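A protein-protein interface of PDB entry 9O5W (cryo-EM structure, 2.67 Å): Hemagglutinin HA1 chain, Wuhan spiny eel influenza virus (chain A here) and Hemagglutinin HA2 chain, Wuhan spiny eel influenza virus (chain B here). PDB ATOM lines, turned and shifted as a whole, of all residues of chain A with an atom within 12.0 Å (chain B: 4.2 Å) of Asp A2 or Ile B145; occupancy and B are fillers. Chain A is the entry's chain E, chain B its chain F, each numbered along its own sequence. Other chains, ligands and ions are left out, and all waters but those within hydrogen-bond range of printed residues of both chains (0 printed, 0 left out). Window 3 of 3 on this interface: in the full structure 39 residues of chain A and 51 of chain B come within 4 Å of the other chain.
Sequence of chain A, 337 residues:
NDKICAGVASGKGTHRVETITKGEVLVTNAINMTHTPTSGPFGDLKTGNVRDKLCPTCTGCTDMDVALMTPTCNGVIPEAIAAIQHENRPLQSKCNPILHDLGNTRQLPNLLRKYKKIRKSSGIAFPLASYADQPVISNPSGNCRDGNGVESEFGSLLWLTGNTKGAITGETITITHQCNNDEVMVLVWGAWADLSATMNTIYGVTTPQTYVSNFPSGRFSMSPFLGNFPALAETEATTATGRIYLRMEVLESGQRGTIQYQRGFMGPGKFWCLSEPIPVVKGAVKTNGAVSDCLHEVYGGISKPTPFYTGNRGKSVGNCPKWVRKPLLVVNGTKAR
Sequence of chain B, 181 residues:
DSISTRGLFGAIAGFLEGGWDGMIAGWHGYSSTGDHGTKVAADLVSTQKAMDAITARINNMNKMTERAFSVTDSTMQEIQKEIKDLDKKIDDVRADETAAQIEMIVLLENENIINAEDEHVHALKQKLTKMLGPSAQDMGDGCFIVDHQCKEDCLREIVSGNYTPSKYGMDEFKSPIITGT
O of Asp A2 touches O of Phe B144, at 3.6 Å.
O of Asp A2 touches CA of Ile B145, 3.3 Å away.
Cys B150 touches Asp A2.
O of Lys A3 touches CA of Ser B32 (3.3 Å).
CA of Lys A3 touches O of Phe B144, 3.3 Å away.
Lys A3 touches Ile B145.
Val B146 touches Ile A4 (CG2 to CD1, 3.8 Å).
SG of Cys B150 touches CD1 of Ile A4 (3.4 Å).
Of chain B, only Ser B32, Thr B33, Gly B34, His B36, Phe B144, Ile B145, Val B146, His B148 and Cys B150 come within 4 Å of Asp A2.
Of the printed residues of chain B, Lys A3 touches Ser B32, Thr B33, Phe B144 and Ile B145.
Printed residues of chain B within 4 Å of Ile A4: Phe B144 (2.8 Å), Val B146 (3.8 Å) and Cys B150 (3.4 Å).
Ser B32 touches two residues of chain A.
Of the printed residues of chain A, Gly B34 touches Asp A2.
His B36 touches just one residue of chain A: Asp A2.
No residue of chain A comes within 4 Å of Ala B136.
No residue of chain A comes within 4 Å of Gln B137.
Of the printed residues of chain A, Phe B144 touches Asp A2, Lys A3 and Ile A4.
Ile B145 touches just these residues of chain A: Asp A2 and Lys A3.
Of chain A, only Asp A2 and Ile A4 come within 4 Å of Val B146.
Of chain A, only Asp A2 comes within 4 Å of His B148.
No residue of chain A comes within 4 Å of Gln B149.
Cys B150 touches just these residues of chain A: Asp A2 and Ile A4.
The nearest residue of chain A that does not touch Ile B145 is Ile A4 (5.0 Å).
The side-chain carboxylate of Asp A2 sits at hydrogen-bond distance from the side-chain hydroxyl of Ser B32 (3.3 Å).
OD1 of Asp A2 lies close to O of Thr B33.
OD1 of Asp A2 sits at hydrogen-bond distance from N of Gly B34, at 3.2 Å.
NE2 of His B36 lies within hydrogen-bond range of OD2 of Asp A2 (2.9 Å).
The backbone carbonyl oxygen (O) of Val B146 lies within hydrogen-bond range of the backbone NH (N) of Asp A2.
The backbone NH (N) of Asp A2 is in hydrogen-bond range of the backbone carbonyl oxygen (O) of His B148 (2.9 Å).
The backbone carbonyl oxygen (O) of Lys A3 lies within hydrogen-bond range of the backbone NH (N) of Thr B33 (3.1 Å).
The backbone carbonyl oxygen (O) of Ile A4 is in hydrogen-bond range of the backbone NH (N) of Phe B144, at 2.8 Å.
A ring nitrogen (NE2) of His B36 is in hydrogen-bond range of the side-chain hydroxyl of Ser B32 (3.5 Å).
O of Cys B150 sits at hydrogen-bond distance from OG of Ser B32, 2.6 Å away.
NE2 of His B36 is in hydrogen-bond range of O of Cys B150, at 2.9 Å.
N of Gln B137 is in hydrogen-bond range of O of Ile B145 (3.2 Å).
Of the 13 printed residues of chain B, 9 touch a printed residue of chain A.
Hydrophobic or aromatic side chains of chain B within 4 Å of the printed part of chain A: His B36, Ile B145 and Val B146.
Along chain B the printed residues that touch a printed residue of chain A span positions 32 to 150.
Printed residues of chain A that touch a printed residue of chain B: Asp A2, Lys A3 and Ile A4.
Among the printed residues, 16 pairs touch across the chains.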
ATOM      1  N   ASP A   2      20.070  29.530  -5.501  1.00  0.00           N
ATOM      2  CA  ASP A   2      20.024  28.131  -5.098  1.00  0.00           C
ATOM      3  C   ASP A   2      18.634  27.576  -5.407  1.00  0.00           C
ATOM      4  O   ASP A   2      17.774  28.329  -5.844  1.00  0.00           O
ATOM      5  CB  ASP A   2      20.352  28.014  -3.613  1.00  0.00           C
ATOM      6  CG  ASP A   2      21.218  26.822  -3.298  1.00  0.00           C
ATOM      7  OD1 ASP A   2      20.771  25.686  -3.537  1.00  0.00           O
ATOM      8  OD2 ASP A   2      22.353  27.024  -2.815  1.00  0.00           O
ATOM      9  N   LYS A   3      18.402  26.284  -5.152  1.00  0.00           N
ATOM     10  CA  LYS A   3      17.118  25.631  -5.415  1.00  0.00           C
ATOM     11  C   LYS A   3      16.510  25.174  -4.097  1.00  0.00           C
ATOM     12  O   LYS A   3      17.034  24.262  -3.453  1.00  0.00           O
ATOM     13  CB  LYS A   3      17.253  24.453  -6.380  1.00  0.00           C
ATOM     14  CG  LYS A   3      15.907  23.796  -6.691  1.00  0.00           C
ATOM     15  CD  LYS A   3      15.961  22.821  -7.853  1.00  0.00           C
ATOM     16  CE  LYS A   3      16.649  21.525  -7.476  1.00  0.00           C
ATOM     17  NZ  LYS A   3      16.521  20.501  -8.546  1.00  0.00           N
ATOM     18  N   ILE A   4      15.390  25.787  -3.721  1.00  0.00           N
ATOM     19  CA  ILE A   4      14.705  25.522  -2.461  1.00  0.00           C
ATOM     20  C   ILE A   4      13.446  24.730  -2.791  1.00  0.00           C
ATOM     21  O   ILE A   4      12.568  25.229  -3.504  1.00  0.00           O
ATOM     22  CB  ILE A   4      14.346  26.831  -1.736  1.00  0.00           C
ATOM     23  CG1 ILE A   4      15.609  27.660  -1.446  1.00  0.00           C
ATOM     24  CG2 ILE A   4      13.603  26.536  -0.419  1.00  0.00           C
ATOM     25  CD1 ILE A   4      15.339  29.096  -0.990  1.00  0.00           C
ATOM     26  N   CYS A   5      13.351  23.504  -2.271  1.00  0.00           N
ATOM     27  CA  CYS A   5      12.238  22.608  -2.561  1.00  0.00           C
ATOM     28  C   CYS A   5      11.429  22.299  -1.311  1.00  0.00           C
ATOM     29  O   CYS A   5      11.966  22.227  -0.202  1.00  0.00           O
ATOM     30  CB  CYS A   5      12.723  21.285  -3.169  1.00  0.00           C
ATOM     31  SG  CYS A   5      13.555  21.435  -4.760  1.00  0.00           S
ATOM     32  N   ALA A   6      10.125  22.124  -1.514  1.00  0.00           N
ATOM     33  CA  ALA A   6       9.202  21.637  -0.501  1.00  0.00           C
ATOM     34  C   ALA A   6       8.734  20.248  -0.908  1.00  0.00           C
ATOM     35  O   ALA A   6       8.515  19.982  -2.093  1.00  0.00           O
ATOM     36  CB  ALA A   6       8.001  22.569  -0.341  1.00  0.00           C
ATOM     37  N   SER B  32      17.617  22.537   0.387  1.00  0.00           N
ATOM     38  CA  SER B  32      18.320  23.481  -0.478  1.00  0.00           C
ATOM     39  C   SER B  32      19.483  22.753  -1.133  1.00  0.00           C
ATOM     40  O   SER B  32      20.407  22.325  -0.437  1.00  0.00           O
ATOM     41  CB  SER B  32      18.820  24.688   0.319  1.00  0.00           C
ATOM     42  OG  SER B  32      19.597  25.548  -0.493  1.00  0.00           O
ATOM     43  N   THR B  33      19.446  22.619  -2.460  1.00  0.00           N
ATOM     44  CA  THR B  33      20.480  21.909  -3.213  1.00  0.00           C
ATOM     45  C   THR B  33      21.214  22.853  -4.156  1.00  0.00           C
ATOM     46  O   THR B  33      20.595  23.458  -5.037  1.00  0.00           O
ATOM     47  CB  THR B  33      19.891  20.731  -4.002  1.00  0.00           C
ATOM     48  OG1 THR B  33      20.865  20.253  -4.939  1.00  0.00           O
ATOM     49  CG2 THR B  33      18.624  21.110  -4.762  1.00  0.00           C
ATOM     50  N   GLY B  34      22.529  22.987  -3.968  1.00  0.00           N
ATOM     51  CA  GLY B  34      23.302  23.891  -4.806  1.00  0.00           C
ATOM     52  C   GLY B  34      24.810  23.723  -4.730  1.00  0.00           C
ATOM     53  O   GLY B  34      25.318  22.599  -4.628  1.00  0.00           O
ATOM     54  N   HIS B  36      26.731  24.117  -2.348  1.00  0.00           N
ATOM     55  CA  HIS B  36      27.082  23.595  -1.039  1.00  0.00           C
ATOM     56  C   HIS B  36      26.505  22.199  -0.849  1.00  0.00           C
ATOM     57  O   HIS B  36      26.476  21.694   0.279  1.00  0.00           O
ATOM     58  CB  HIS B  36      26.569  24.519   0.075  1.00  0.00           C
ATOM     59  CG  HIS B  36      25.100  24.819  -0.006  1.00  0.00           C
ATOM     60  ND1 HIS B  36      24.174  24.209   0.807  1.00  0.00           N
ATOM     61  CD2 HIS B  36      24.405  25.689  -0.780  1.00  0.00           C
ATOM     62  CE1 HIS B  36      22.967  24.658   0.513  1.00  0.00           C
ATOM     63  NE2 HIS B  36      23.080  25.563  -0.441  1.00  0.00           N
ATOM     64  N   ALA B 136      11.482  34.714  -7.383  1.00  0.00           N
ATOM     65  CA  ALA B 136      11.784  33.292  -7.366  1.00  0.00           C
ATOM     66  C   ALA B 136      11.097  32.641  -8.558  1.00  0.00           C
ATOM     67  O   ALA B 136       9.952  32.972  -8.880  1.00  0.00           O
ATOM     68  CB  ALA B 136      11.316  32.656  -6.060  1.00  0.00           C
ATOM     69  N   GLN B 137      11.784  31.713  -9.219  1.00  0.00           N
ATOM     70  CA  GLN B 137      11.199  31.015 -10.358  1.00  0.00           C
ATOM     71  C   GLN B 137      10.486  29.768  -9.857  1.00  0.00           C
ATOM     72  O   GLN B 137      11.115  28.883  -9.278  1.00  0.00           O
ATOM     73  CB  GLN B 137      12.282  30.641 -11.366  1.00  0.00           C
ATOM     74  CG  GLN B 137      13.004  31.831 -11.962  1.00  0.00           C
ATOM     75  CD  GLN B 137      14.024  31.431 -13.004  1.00  0.00           C
ATOM     76  OE1 GLN B 137      14.627  30.361 -12.922  1.00  0.00           O
ATOM     77  NE2 GLN B 137      14.222  32.289 -13.996  1.00  0.00           N
ATOM     78  N   MET B 139       9.151  26.329 -10.384  1.00  0.00           N
ATOM     79  CA  MET B 139       9.437  25.267 -11.339  1.00  0.00           C
ATOM     80  C   MET B 139       8.287  24.279 -11.513  1.00  0.00           C
ATOM     81  O   MET B 139       8.400  23.373 -12.342  1.00  0.00           O
ATOM     82  CB  MET B 139      10.700  24.518 -10.902  1.00  0.00           C
ATOM     83  CG  MET B 139      11.939  25.422 -10.813  1.00  0.00           C
ATOM     84  SD  MET B 139      13.591  24.766 -11.194  1.00  0.00           S
ATOM     85  CE  MET B 139      13.419  22.980 -11.167  1.00  0.00           C
ATOM     86  N   PHE B 144      11.839  26.152  -6.012  1.00  0.00           N
ATOM     87  CA  PHE B 144      12.034  27.519  -6.462  1.00  0.00           C
ATOM     88  C   PHE B 144      13.518  27.801  -6.582  1.00  0.00           C
ATOM     89  O   PHE B 144      14.323  27.295  -5.798  1.00  0.00           O
ATOM     90  CB  PHE B 144      11.408  28.508  -5.486  1.00  0.00           C
ATOM     91  CG  PHE B 144       9.919  28.389  -5.373  1.00  0.00           C
ATOM     92  CD1 PHE B 144       9.350  27.429  -4.557  1.00  0.00           C
ATOM     93  CD2 PHE B 144       9.089  29.253  -6.061  1.00  0.00           C
ATOM     94  CE1 PHE B 144       7.985  27.324  -4.445  1.00  0.00           C
ATOM     95  CE2 PHE B 144       7.725  29.146  -5.955  1.00  0.00           C
ATOM     96  CZ  PHE B 144       7.173  28.181  -5.144  1.00  0.00           C
ATOM     97  N   ILE B 145      13.869  28.635  -7.560  1.00  0.00           N
ATOM     98  CA  ILE B 145      15.237  29.094  -7.762  1.00  0.00           C
ATOM     99  C   ILE B 145      15.343  30.541  -7.304  1.00  0.00           C
ATOM    100  O   ILE B 145      14.557  31.394  -7.734  1.00  0.00           O
ATOM    101  CB  ILE B 145      15.668  28.951  -9.235  1.00  0.00           C
ATOM    102  CG1 ILE B 145      15.446  27.520  -9.758  1.00  0.00           C
ATOM    103  CG2 ILE B 145      17.138  29.357  -9.419  1.00  0.00           C
ATOM    104  CD1 ILE B 145      16.234  26.424  -9.057  1.00  0.00           C
ATOM    105  N   VAL B 146      16.312  30.813  -6.432  1.00  0.00           N
ATOM    106  CA  VAL B 146      16.567  32.141  -5.887  1.00  0.00           C
ATOM    107  C   VAL B 146      18.016  32.478  -6.209  1.00  0.00           C
ATOM    108  O   VAL B 146      18.880  31.597  -6.152  1.00  0.00           O
ATOM    109  CB  VAL B 146      16.280  32.190  -4.369  1.00  0.00           C
ATOM    110  CG1 VAL B 146      14.815  31.879  -4.100  1.00  0.00           C
ATOM    111  CG2 VAL B 146      17.153  31.190  -3.603  1.00  0.00           C
ATOM    112  N   HIS B 148      20.663  33.516  -4.796  1.00  0.00           N
ATOM    113  CA  HIS B 148      21.534  33.671  -3.637  1.00  0.00           C
ATOM    114  C   HIS B 148      21.853  32.275  -3.131  1.00  0.00           C
ATOM    115  O   HIS B 148      21.179  31.307  -3.495  1.00  0.00           O
ATOM    116  CB  HIS B 148      20.910  34.529  -2.535  1.00  0.00           C
ATOM    117  CG  HIS B 148      19.751  33.886  -1.849  1.00  0.00           C
ATOM    118  ND1 HIS B 148      19.905  33.055  -0.761  1.00  0.00           N
ATOM    119  CD2 HIS B 148      18.421  33.960  -2.081  1.00  0.00           C
ATOM    120  CE1 HIS B 148      18.720  32.635  -0.361  1.00  0.00           C
ATOM    121  NE2 HIS B 148      17.803  33.169  -1.145  1.00  0.00           N
ATOM    122  N   GLN B 149      22.879  32.167  -2.289  1.00  0.00           N
ATOM    123  CA  GLN B 149      23.165  30.881  -1.668  1.00  0.00           C
ATOM    124  C   GLN B 149      22.247  30.741  -0.459  1.00  0.00           C
ATOM    125  O   GLN B 149      22.059  31.687   0.311  1.00  0.00           O
ATOM    126  CB  GLN B 149      24.640  30.762  -1.276  1.00  0.00           C
ATOM    127  CG  GLN B 149      24.933  29.766  -0.156  1.00  0.00           C
ATOM    128  CD  GLN B 149      26.329  29.182  -0.247  1.00  0.00           C
ATOM    129  OE1 GLN B 149      26.501  27.964  -0.202  1.00  0.00           O
ATOM    130  NE2 GLN B 149      27.327  30.042  -0.401  1.00  0.00           N
ATOM    131  N   CYS B 150      21.678  29.549  -0.299  1.00  0.00           N
ATOM    132  CA  CYS B 150      20.752  29.214   0.782  1.00  0.00           C
ATOM    133  C   CYS B 150      21.367  28.043   1.545  1.00  0.00           C
ATOM    134  O   CYS B 150      21.127  26.887   1.193  1.00  0.00           O
ATOM    135  CB  CYS B 150      19.375  28.883   0.148  1.00  0.00           C
ATOM    136  SG  CYS B 150      17.907  28.532   1.176  1.00  0.00           S
